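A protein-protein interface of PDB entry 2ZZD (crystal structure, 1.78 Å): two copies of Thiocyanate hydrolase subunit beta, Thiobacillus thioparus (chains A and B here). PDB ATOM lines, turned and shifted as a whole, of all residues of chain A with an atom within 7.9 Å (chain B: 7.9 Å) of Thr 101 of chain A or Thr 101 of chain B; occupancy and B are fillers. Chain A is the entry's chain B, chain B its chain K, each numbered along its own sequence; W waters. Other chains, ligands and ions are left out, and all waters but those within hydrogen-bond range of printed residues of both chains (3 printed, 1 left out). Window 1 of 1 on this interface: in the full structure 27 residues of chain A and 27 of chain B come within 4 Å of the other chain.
O of Thr 27 of chain B sits close to O of Leu 104 of chain A. The backbone carbonyl oxygen (O) of Thr 27 of chain A sits close to the backbone carbonyl oxygen (O) of Leu 104 of chain B (3.2 Å). The side-chain hydroxyl (OG1) of Thr 101 of chain A is in hydrogen-bond range of the side-chain hydroxyl (OG1) of Thr 101 of chain B (2.8 Å). The backbone NH (N) of Ala 29 of chain B lies within hydrogen-bond range of the backbone carbonyl oxygen (O) of Leu 104 of chain A. The backbone NH (N) of Ala 29 of chain A is in hydrogen-bond range of the backbone carbonyl oxygen (O) of Leu 104 of chain B, at 2.7 Å.
The side-chain amide nitrogen (NE2) of Gln 100 of chain B lies close to the guanidinium group (NH1) of Arg 45 of chain B (3.0 Å). The guanidinium group (NH1) of Arg 45 of chain A lies close to the side-chain amide nitrogen (NE2) of Gln 100 of chain A (3.0 Å).
Gly 105 of chain B touches Thr 27 of chain A (CA to OG1, 3.6 Å). CA of Ala 29 of chain A touches O of Met 106 of chain B, 3.6 Å away. Leu 104 of chain B touches Pro 30 of chain A. CD of Pro 30 of chain A touches O of Gly 105 of chain B, 3.3 Å away. CD of Pro 30 of chain A touches O of Met 106 of chain B, at 3.9 Å. Gln 100 of chain A touches Thr 101 of chain B. Leu 104 of chain A touches Pro 30 of chain B (O to CD, 3.4 Å). Gly 105 of chain A touches Pro 30 of chain B (O to CD, 3.4 Å). O of Met 106 of chain A touches CA of Ala 29 of chain B (3.6 Å). Met 106 of chain A touches Pro 30 of chain B (O to CD, 3.96 Å).
Arg 45 of chain A touches none of the printed residues of chain B. Of chain B, only Gln 100 and Thr 101 come within 4 Å of Thr 101 of chain A. Of the printed residues of chain B, Leu 104 of chain A touches Thr 27 (3.2 Å), Ala 29 (2.8 Å) and Pro 30 (3.4 Å). Of the printed residues of chain B, Gly 105 of chain A touches Thr 27, Pro 30 and Tyr 43. Of the printed residues of chain B, Met 106 of chain A touches Ala 29, Pro 30 and Tyr 43. Of the printed residues of chain A, Tyr 43 of chain B touches Val 102, Gly 105 and Met 106. Of chain A, only Gln 100 (3.6 Å) and Thr 101 (2.8 Å) come within 4 Å of Thr 101 of chain B. The nearest residue of chain B that does not touch Thr 101 of chain A is Tyr 43 of chain B (4.02 Å). The nearest residue of chain A that does not touch Thr 101 of chain B is Tyr 43 of chain A (4.1 Å). The nearest printed residue of chain B that does not touch Gly 105 of chain A is Ala 29 of chain B (4.9 Å).
Hydrophobic or aromatic side chains of chain A that line the printed part of chain B: Pro 30, Tyr 43, Val 102, Leu 104 and Met 106. Among the printed residues, 23 pairs touch across the chains. Among the printed residues, no Asp or Glu carboxylate lies within 4 Å of a Lys or Arg side-chain nitrogen of the other chain.
Thr 27 of chain A touches Gly 105 of chain B, and with the chains exchanged Gly 105 of chain A touches Thr 27 of chain B. Pro 30 of chain A touches Gly 105 of chain B, and with the chains exchanged Gly 105 of chain A touches Pro 30 of chain B. Tyr 43 of chain A touches Val 102 of chain B, and with the chains exchanged Val 102 of chain A touches Tyr 43 of chain B. Tyr 43 of chain A touches Met 106 of chain B, and with the chains exchanged Met 106 of chain A touches Tyr 43 of chain B.
Water W1 lies within hydrogen-bond range of the backbone carbonyl oxygen (O) of Gly 105 of chain B (2.8 Å) and the side-chain hydroxyl (OH) of Tyr 43 of chain A (2.8 Å). Water W2 bridges O of Gly 105 of chain A (2.8 Å) and OH of Tyr 43 of chain B (2.9 Å). Water W3 lies within hydrogen-bond range of the backbone carbonyl oxygen (O) of Val 98 of chain B, the backbone carbonyl oxygen (O) of Val 98 of chain A, the backbone NH (N) of Gly 99 of chain A and the backbone NH (N) of Gly 99 of chain B.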
ATOM      1  N   THR A  27      13.959  30.763   8.060  1.00  0.00           N
ATOM      2  CA  THR A  27      13.165  31.960   7.815  1.00  0.00           C
ATOM      3  C   THR A  27      13.711  33.083   8.690  1.00  0.00           C
ATOM      4  O   THR A  27      13.770  32.942   9.911  1.00  0.00           O
ATOM      5  CB  THR A  27      11.676  31.736   8.163  1.00  0.00           C
ATOM      6  OG1 THR A  27      11.556  31.295   9.522  1.00  0.00           O
ATOM      7  CG2 THR A  27      11.070  30.692   7.239  1.00  0.00           C
ATOM      8  N   ALA A  29      12.699  36.731   9.111  1.00  0.00           N
ATOM      9  CA  ALA A  29      11.831  37.894   8.932  1.00  0.00           C
ATOM     10  C   ALA A  29      11.605  38.204   7.454  1.00  0.00           C
ATOM     11  O   ALA A  29      11.981  39.272   6.971  1.00  0.00           O
ATOM     12  CB  ALA A  29      12.432  39.113   9.641  1.00  0.00           C
ATOM     13  N   PRO A  30      10.978  37.270   6.717  1.00  0.00           N
ATOM     14  CA  PRO A  30      10.702  37.452   5.286  1.00  0.00           C
ATOM     15  C   PRO A  30       9.790  38.648   5.044  1.00  0.00           C
ATOM     16  O   PRO A  30       9.016  39.032   5.920  1.00  0.00           O
ATOM     17  CB  PRO A  30       9.999  36.155   4.883  1.00  0.00           C
ATOM     18  CG  PRO A  30      10.328  35.181   5.977  1.00  0.00           C
ATOM     19  CD  PRO A  30      10.376  36.023   7.218  1.00  0.00           C
ATOM     20  N   ALA A  42      -1.044  29.300   8.560  1.00  0.00           N
ATOM     21  CA  ALA A  42      -0.222  28.383   9.344  1.00  0.00           C
ATOM     22  C   ALA A  42       0.522  29.097  10.476  1.00  0.00           C
ATOM     23  O   ALA A  42       0.634  28.567  11.582  1.00  0.00           O
ATOM     24  CB  ALA A  42       0.770  27.661   8.434  1.00  0.00           C
ATOM     25  N   TYR A  43       1.034  30.295  10.205  1.00  0.00           N
ATOM     26  CA  TYR A  43       1.755  31.053  11.229  1.00  0.00           C
ATOM     27  C   TYR A  43       0.839  31.633  12.303  1.00  0.00           C
ATOM     28  O   TYR A  43       1.235  31.733  13.468  1.00  0.00           O
ATOM     29  CB  TYR A  43       2.551  32.199  10.597  1.00  0.00           C
ATOM     30  CG  TYR A  43       3.877  31.790  10.007  1.00  0.00           C
ATOM     31  CD1 TYR A  43       4.146  31.979   8.649  1.00  0.00           C
ATOM     32  CD2 TYR A  43       4.872  31.221  10.806  1.00  0.00           C
ATOM     33  CE1 TYR A  43       5.370  31.609   8.103  1.00  0.00           C
ATOM     34  CE2 TYR A  43       6.100  30.848  10.269  1.00  0.00           C
ATOM     35  CZ  TYR A  43       6.341  31.044   8.916  1.00  0.00           C
ATOM     36  OH  TYR A  43       7.542  30.662   8.366  1.00  0.00           O
ATOM     37  N   ARG A  45      -1.943  30.315  13.263  1.00  0.00           N
ATOM     38  CA  ARG A  45      -2.703  29.190  13.805  1.00  0.00           C
ATOM     39  C   ARG A  45      -2.674  29.268  15.328  1.00  0.00           C
ATOM     40  O   ARG A  45      -1.816  29.930  15.899  1.00  0.00           O
ATOM     41  CB  ARG A  45      -2.010  27.879  13.433  1.00  0.00           C
ATOM     42  CG  ARG A  45      -0.680  27.748  14.192  1.00  0.00           C
ATOM     43  CD  ARG A  45      -0.029  26.381  14.096  1.00  0.00           C
ATOM     44  NE  ARG A  45      -0.956  25.298  14.400  1.00  0.00           N
ATOM     45  CZ  ARG A  45      -0.592  24.025  14.532  1.00  0.00           C
ATOM     46  NH1 ARG A  45       0.682  23.681  14.397  1.00  0.00           N
ATOM     47  NH2 ARG A  45      -1.503  23.093  14.767  1.00  0.00           N
ATOM     48  N   PRO A  47      -1.673  27.200  18.249  1.00  0.00           N
ATOM     49  CA  PRO A  47      -0.823  26.023  18.481  1.00  0.00           C
ATOM     50  C   PRO A  47      -1.446  24.731  19.009  1.00  0.00           C
ATOM     51  O   PRO A  47      -1.028  23.639  18.621  1.00  0.00           O
ATOM     52  CB  PRO A  47       0.251  26.555  19.436  1.00  0.00           C
ATOM     53  CG  PRO A  47       0.349  27.987  19.065  1.00  0.00           C
ATOM     54  CD  PRO A  47      -1.102  28.381  18.919  1.00  0.00           C
ATOM     55  N   VAL A  98       1.708  30.897  24.286  1.00  0.00           N
ATOM     56  CA  VAL A  98       3.130  30.571  24.415  1.00  0.00           C
ATOM     57  C   VAL A  98       3.846  30.464  23.073  1.00  0.00           C
ATOM     58  O   VAL A  98       5.072  30.571  23.008  1.00  0.00           O
ATOM     59  CB  VAL A  98       3.364  29.264  25.210  1.00  0.00           C
ATOM     60  CG1 VAL A  98       2.909  29.442  26.644  1.00  0.00           C
ATOM     61  CG2 VAL A  98       2.634  28.107  24.552  1.00  0.00           C
ATOM     62  N   GLY A  99       3.083  30.258  22.004  1.00  0.00           N
ATOM     63  CA  GLY A  99       3.678  30.167  20.680  1.00  0.00           C
ATOM     64  C   GLY A  99       4.159  28.775  20.314  1.00  0.00           C
ATOM     65  O   GLY A  99       4.455  27.959  21.178  1.00  0.00           O
ATOM     66  N   GLN A 100       4.255  28.530  19.012  1.00  0.00           N
ATOM     67  CA  GLN A 100       4.657  27.236  18.462  1.00  0.00           C
ATOM     68  C   GLN A 100       5.898  26.565  19.059  1.00  0.00           C
ATOM     69  O   GLN A 100       5.848  25.393  19.437  1.00  0.00           O
ATOM     70  CB  GLN A 100       4.854  27.363  16.951  1.00  0.00           C
ATOM     71  CG  GLN A 100       5.145  26.047  16.238  1.00  0.00           C
ATOM     72  CD  GLN A 100       3.955  25.104  16.252  1.00  0.00           C
ATOM     73  OE1 GLN A 100       3.701  24.406  17.236  1.00  0.00           O
ATOM     74  NE2 GLN A 100       3.210  25.092  15.158  1.00  0.00           N
ATOM     75  N   THR A 101       7.010  27.295  19.133  1.00  0.00           N
ATOM     76  CA  THR A 101       8.256  26.726  19.643  1.00  0.00           C
ATOM     77  C   THR A 101       8.179  26.218  21.079  1.00  0.00           C
ATOM     78  O   THR A 101       8.507  25.056  21.356  1.00  0.00           O
ATOM     79  CB  THR A 101       9.417  27.736  19.521  1.00  0.00           C
ATOM     80  OG1 THR A 101       9.669  28.005  18.136  1.00  0.00           O
ATOM     81  CG2 THR A 101      10.690  27.173  20.147  1.00  0.00           C
ATOM     82  N   VAL A 102       7.768  27.082  21.998  1.00  0.00           N
ATOM     83  CA  VAL A 102       7.665  26.679  23.395  1.00  0.00           C
ATOM     84  C   VAL A 102       6.572  25.622  23.562  1.00  0.00           C
ATOM     85  O   VAL A 102       6.693  24.706  24.373  1.00  0.00           O
ATOM     86  CB  VAL A 102       7.356  27.898  24.300  1.00  0.00           C
ATOM     87  CG1 VAL A 102       6.899  27.437  25.680  1.00  0.00           C
ATOM     88  CG2 VAL A 102       8.607  28.760  24.445  1.00  0.00           C
ATOM     89  N   TYR A 103       5.507  25.743  22.777  1.00  0.00           N
ATOM     90  CA  TYR A 103       4.404  24.797  22.867  1.00  0.00           C
ATOM     91  C   TYR A 103       4.845  23.340  22.716  1.00  0.00           C
ATOM     92  O   TYR A 103       4.339  22.460  23.419  1.00  0.00           O
ATOM     93  CB  TYR A 103       3.339  25.111  21.812  1.00  0.00           C
ATOM     94  CG  TYR A 103       2.117  24.242  21.965  1.00  0.00           C
ATOM     95  CD1 TYR A 103       1.338  24.314  23.119  1.00  0.00           C
ATOM     96  CD2 TYR A 103       1.769  23.302  20.991  1.00  0.00           C
ATOM     97  CE1 TYR A 103       0.245  23.471  23.307  1.00  0.00           C
ATOM     98  CE2 TYR A 103       0.677  22.449  21.173  1.00  0.00           C
ATOM     99  CZ  TYR A 103      -0.076  22.538  22.333  1.00  0.00           C
ATOM    100  OH  TYR A 103      -1.129  21.674  22.532  1.00  0.00           O
ATOM    101  N   LEU A 104       5.783  23.076  21.811  1.00  0.00           N
ATOM    102  CA  LEU A 104       6.242  21.705  21.600  1.00  0.00           C
ATOM    103  C   LEU A 104       7.661  21.422  22.094  1.00  0.00           C
ATOM    104  O   LEU A 104       8.057  20.259  22.221  1.00  0.00           O
ATOM    105  CB  LEU A 104       6.121  21.345  20.114  1.00  0.00           C
ATOM    106  CG  LEU A 104       4.676  21.160  19.639  1.00  0.00           C
ATOM    107  CD1 LEU A 104       4.609  21.043  18.117  1.00  0.00           C
ATOM    108  CD2 LEU A 104       4.100  19.915  20.299  1.00  0.00           C
ATOM    109  N   GLY A 105       8.417  22.476  22.384  1.00  0.00           N
ATOM    110  CA  GLY A 105       9.781  22.299  22.854  1.00  0.00           C
ATOM    111  C   GLY A 105       9.892  22.102  24.356  1.00  0.00           C
ATOM    112  O   GLY A 105      10.813  21.438  24.835  1.00  0.00           O
ATOM    113  N   MET A 106       8.959  22.682  25.105  1.00  0.00           N
ATOM    114  CA  MET A 106       8.973  22.569  26.559  1.00  0.00           C
ATOM    115  C   MET A 106       7.993  21.507  27.054  1.00  0.00           C
ATOM    116  O   MET A 106       7.129  21.049  26.304  1.00  0.00           O
ATOM    117  CB  MET A 106       8.643  23.929  27.178  1.00  0.00           C
ATOM    118  CG  MET A 106       9.789  24.937  27.077  1.00  0.00           C
ATOM    119  SD  MET A 106      11.154  24.554  28.216  1.00  0.00           S
ATOM    120  CE  MET A 106      10.571  25.422  29.693  1.00  0.00           C
ATOM    121  N   ARG A 111       4.766  24.409  30.758  1.00  0.00           N
ATOM    122  CA  ARG A 111       3.905  25.448  30.209  1.00  0.00           C
ATOM    123  C   ARG A 111       2.856  25.876  31.242  1.00  0.00           C
ATOM    124  O   ARG A 111       2.528  27.059  31.350  1.00  0.00           O
ATOM    125  CB  ARG A 111       3.235  24.957  28.920  1.00  0.00           C
ATOM    126  CG  ARG A 111       4.237  24.696  27.802  1.00  0.00           C
ATOM    127  CD  ARG A 111       3.573  24.331  26.471  1.00  0.00           C
ATOM    128  NE  ARG A 111       2.821  23.079  26.528  1.00  0.00           N
ATOM    129  CZ  ARG A 111       1.508  22.998  26.726  1.00  0.00           C
ATOM    130  NH1 ARG A 111       0.786  24.099  26.889  1.00  0.00           N
ATOM    131  NH2 ARG A 111       0.911  21.813  26.755  1.00  0.00           N
ATOM    132  N   THR B  27      11.042  18.048  18.441  1.00  0.00           N
ATOM    133  CA  THR B  27      10.693  18.062  19.857  1.00  0.00           C
ATOM    134  C   THR B  27       9.178  17.987  19.983  1.00  0.00           C
ATOM    135  O   THR B  27       8.461  18.830  19.443  1.00  0.00           O
ATOM    136  CB  THR B  27      11.197  19.343  20.546  1.00  0.00           C
ATOM    137  OG1 THR B  27      10.659  20.491  19.876  1.00  0.00           O
ATOM    138  CG2 THR B  27      12.720  19.393  20.514  1.00  0.00           C
ATOM    139  N   ALA B  29       6.911  17.884  23.012  1.00  0.00           N
ATOM    140  CA  ALA B  29       6.599  17.990  24.435  1.00  0.00           C
ATOM    141  C   ALA B  29       7.430  17.038  25.298  1.00  0.00           C
ATOM    142  O   ALA B  29       6.889  16.160  25.971  1.00  0.00           O
ATOM    143  CB  ALA B  29       5.098  17.737  24.660  1.00  0.00           C
ATOM    144  N   PRO B  30       8.762  17.217  25.299  1.00  0.00           N
ATOM    145  CA  PRO B  30       9.689  16.385  26.074  1.00  0.00           C
ATOM    146  C   PRO B  30       9.376  16.458  27.566  1.00  0.00           C
ATOM    147  O   PRO B  30       8.816  17.445  28.035  1.00  0.00           O
ATOM    148  CB  PRO B  30      11.057  17.004  25.774  1.00  0.00           C
ATOM    149  CG  PRO B  30      10.853  17.746  24.486  1.00  0.00           C
ATOM    150  CD  PRO B  30       9.479  18.327  24.651  1.00  0.00           C
ATOM    151  N   ALA B  42      17.379  28.817  26.953  1.00  0.00           N
ATOM    152  CA  ALA B  42      17.169  29.052  25.526  1.00  0.00           C
ATOM    153  C   ALA B  42      15.685  29.113  25.151  1.00  0.00           C
ATOM    154  O   ALA B  42      15.289  29.910  24.302  1.00  0.00           O
ATOM    155  CB  ALA B  42      17.870  27.973  24.711  1.00  0.00           C
ATOM    156  N   TYR B  43      14.866  28.261  25.762  1.00  0.00           N
ATOM    157  CA  TYR B  43      13.436  28.266  25.460  1.00  0.00           C
ATOM    158  C   TYR B  43      12.706  29.454  26.067  1.00  0.00           C
ATOM    159  O   TYR B  43      11.758  29.964  25.473  1.00  0.00           O
ATOM    160  CB  TYR B  43      12.759  26.977  25.947  1.00  0.00           C
ATOM    161  CG  TYR B  43      12.906  25.812  25.000  1.00  0.00           C
ATOM    162  CD1 TYR B  43      12.422  25.885  23.694  1.00  0.00           C
ATOM    163  CD2 TYR B  43      13.542  24.639  25.405  1.00  0.00           C
ATOM    164  CE1 TYR B  43      12.573  24.819  22.808  1.00  0.00           C
ATOM    165  CE2 TYR B  43      13.699  23.569  24.534  1.00  0.00           C
ATOM    166  CZ  TYR B  43      13.214  23.664  23.238  1.00  0.00           C
ATOM    167  OH  TYR B  43      13.389  22.613  22.371  1.00  0.00           O
ATOM    168  N   ARG B  45      14.030  32.375  26.643  1.00  0.00           N
ATOM    169  CA  ARG B  45      14.705  33.577  26.153  1.00  0.00           C
ATOM    170  C   ARG B  45      13.654  34.565  25.663  1.00  0.00           C
ATOM    171  O   ARG B  45      12.530  34.174  25.359  1.00  0.00           O
ATOM    172  CB  ARG B  45      15.544  33.230  24.923  1.00  0.00           C
ATOM    173  CG  ARG B  45      14.630  32.899  23.722  1.00  0.00           C
ATOM    174  CD  ARG B  45      15.349  32.789  22.386  1.00  0.00           C
ATOM    175  NE  ARG B  45      16.273  33.893  22.149  1.00  0.00           N
ATOM    176  CZ  ARG B  45      16.909  34.105  21.002  1.00  0.00           C
ATOM    177  NH1 ARG B  45      16.716  33.294  19.969  1.00  0.00           N
ATOM    178  NH2 ARG B  45      17.763  35.109  20.899  1.00  0.00           N
ATOM    179  N   PRO B  47      12.775  36.437  22.590  1.00  0.00           N
ATOM    180  CA  PRO B  47      13.119  36.367  21.163  1.00  0.00           C
ATOM    181  C   PRO B  47      13.859  37.532  20.515  1.00  0.00           C
ATOM    182  O   PRO B  47      14.672  37.321  19.618  1.00  0.00           O
ATOM    183  CB  PRO B  47      11.769  36.133  20.488  1.00  0.00           C
ATOM    184  CG  PRO B  47      10.988  35.417  21.524  1.00  0.00           C
ATOM    185  CD  PRO B  47      11.338  36.169  22.782  1.00  0.00           C
ATOM    186  N   VAL B  98       5.151  37.305  21.008  1.00  0.00           N
ATOM    187  CA  VAL B  98       4.751  36.551  19.816  1.00  0.00           C
ATOM    188  C   VAL B  98       5.421  35.182  19.719  1.00  0.00           C
ATOM    189  O   VAL B  98       4.943  34.304  19.002  1.00  0.00           O
ATOM    190  CB  VAL B  98       5.027  37.335  18.506  1.00  0.00           C
ATOM    191  CG1 VAL B  98       4.161  38.586  18.457  1.00  0.00           C
ATOM    192  CG2 VAL B  98       6.499  37.704  18.405  1.00  0.00           C
ATOM    193  N   GLY B  99       6.529  35.002  20.432  1.00  0.00           N
ATOM    194  CA  GLY B  99       7.218  33.718  20.411  1.00  0.00           C
ATOM    195  C   GLY B  99       8.218  33.554  19.281  1.00  0.00           C
ATOM    196  O   GLY B  99       8.113  34.201  18.244  1.00  0.00           O
ATOM    197  N   GLN B 100       9.174  32.654  19.488  1.00  0.00           N
ATOM    198  CA  GLN B 100      10.246  32.385  18.533  1.00  0.00           C
ATOM    199  C   GLN B 100       9.842  32.152  17.072  1.00  0.00           C
ATOM    200  O   GLN B 100      10.408  32.771  16.168  1.00  0.00           O
ATOM    201  CB  GLN B 100      11.072  31.186  19.015  1.00  0.00           C
ATOM    202  CG  GLN B 100      12.304  30.867  18.168  1.00  0.00           C
ATOM    203  CD  GLN B 100      13.362  31.956  18.230  1.00  0.00           C
ATOM    204  OE1 GLN B 100      13.247  32.996  17.575  1.00  0.00           O
ATOM    205  NE2 GLN B 100      14.396  31.726  19.034  1.00  0.00           N
ATOM    206  N   THR B 101       8.880  31.260  16.834  1.00  0.00           N
ATOM    207  CA  THR B 101       8.469  30.943  15.466  1.00  0.00           C
ATOM    208  C   THR B 101       7.923  32.131  14.677  1.00  0.00           C
ATOM    209  O   THR B 101       8.404  32.432  13.581  1.00  0.00           O
ATOM    210  CB  THR B 101       7.431  29.799  15.446  1.00  0.00           C
ATOM    211  OG1 THR B 101       8.044  28.600  15.936  1.00  0.00           O
ATOM    212  CG2 THR B 101       6.927  29.549  14.024  1.00  0.00           C
ATOM    213  N   VAL B 102       6.910  32.796  15.217  1.00  0.00           N
ATOM    214  CA  VAL B 102       6.331  33.948  14.537  1.00  0.00           C
ATOM    215  C   VAL B 102       7.332  35.102  14.469  1.00  0.00           C
ATOM    216  O   VAL B 102       7.366  35.862  13.493  1.00  0.00           O
ATOM    217  CB  VAL B 102       5.043  34.413  15.257  1.00  0.00           C
ATOM    218  CG1 VAL B 102       4.631  35.808  14.772  1.00  0.00           C
ATOM    219  CG2 VAL B 102       3.919  33.418  14.975  1.00  0.00           C
ATOM    220  N   TYR B 103       8.165  35.222  15.497  1.00  0.00           N
ATOM    221  CA  TYR B 103       9.141  36.299  15.536  1.00  0.00           C
ATOM    222  C   TYR B 103      10.044  36.332  14.304  1.00  0.00           C
ATOM    223  O   TYR B 103      10.375  37.409  13.804  1.00  0.00           O
ATOM    224  CB  TYR B 103      10.006  36.202  16.796  1.00  0.00           C
ATOM    225  CG  TYR B 103      10.929  37.387  16.938  1.00  0.00           C
ATOM    226  CD1 TYR B 103      10.414  38.670  17.131  1.00  0.00           C
ATOM    227  CD2 TYR B 103      12.312  37.242  16.819  1.00  0.00           C
ATOM    228  CE1 TYR B 103      11.251  39.777  17.195  1.00  0.00           C
ATOM    229  CE2 TYR B 103      13.156  38.347  16.880  1.00  0.00           C
ATOM    230  CZ  TYR B 103      12.620  39.610  17.065  1.00  0.00           C
ATOM    231  OH  TYR B 103      13.450  40.704  17.099  1.00  0.00           O
ATOM    232  N   LEU B 104      10.435  35.162  13.809  1.00  0.00           N
ATOM    233  CA  LEU B 104      11.308  35.111  12.642  1.00  0.00           C
ATOM    234  C   LEU B 104      10.636  34.595  11.372  1.00  0.00           C
ATOM    235  O   LEU B 104      11.168  34.771  10.277  1.00  0.00           O
ATOM    236  CB  LEU B 104      12.547  34.268  12.962  1.00  0.00           C
ATOM    237  CG  LEU B 104      13.532  34.965  13.908  1.00  0.00           C
ATOM    238  CD1 LEU B 104      14.603  33.990  14.382  1.00  0.00           C
ATOM    239  CD2 LEU B 104      14.166  36.152  13.189  1.00  0.00           C
ATOM    240  N   GLY B 105       9.466  33.976  11.517  1.00  0.00           N
ATOM    241  CA  GLY B 105       8.759  33.446  10.360  1.00  0.00           C
ATOM    242  C   GLY B 105       7.899  34.463   9.625  1.00  0.00           C
ATOM    243  O   GLY B 105       7.725  34.375   8.404  1.00  0.00           O
ATOM    244  N   MET B 106       7.355  35.426  10.364  1.00  0.00           N
ATOM    245  CA  MET B 106       6.501  36.456   9.776  1.00  0.00           C
ATOM    246  C   MET B 106       7.277  37.741   9.518  1.00  0.00           C
ATOM    247  O   MET B 106       8.396  37.909  10.005  1.00  0.00           O
ATOM    248  CB  MET B 106       5.315  36.738  10.701  1.00  0.00           C
ATOM    249  CG  MET B 106       4.286  35.610  10.744  1.00  0.00           C
ATOM    250  SD  MET B 106       3.265  35.548   9.243  1.00  0.00           S
ATOM    251  CE  MET B 106       2.014  36.751   9.684  1.00  0.00           C
ATOM    252  N   ARG B 111       4.153  41.589  12.381  1.00  0.00           N
ATOM    253  CA  ARG B 111       4.144  41.492  13.835  1.00  0.00           C
ATOM    254  C   ARG B 111       3.569  42.765  14.458  1.00  0.00           C
ATOM    255  O   ARG B 111       2.837  42.702  15.442  1.00  0.00           O
ATOM    256  CB  ARG B 111       5.560  41.221  14.357  1.00  0.00           C
ATOM    257  CG  ARG B 111       6.087  39.856  13.922  1.00  0.00           C
ATOM    258  CD  ARG B 111       7.437  39.494  14.537  1.00  0.00           C
ATOM    259  NE  ARG B 111       8.511  40.397  14.130  1.00  0.00           N
ATOM    260  CZ  ARG B 111       8.943  41.422  14.861  1.00  0.00           C
ATOM    261  NH1 ARG B 111       8.392  41.683  16.041  1.00  0.00           N
ATOM    262  NH2 ARG B 111       9.940  42.179  14.420  1.00  0.00           N
HETATM  263  O   HOH W   1       8.147  32.520   6.376  1.00  0.00           O
HETATM  264  O   HOH W   2      13.229  20.255  23.991  1.00  0.00           O
HETATM  265  O   HOH W   3       4.179  33.201  21.646  1.00  0.00           O
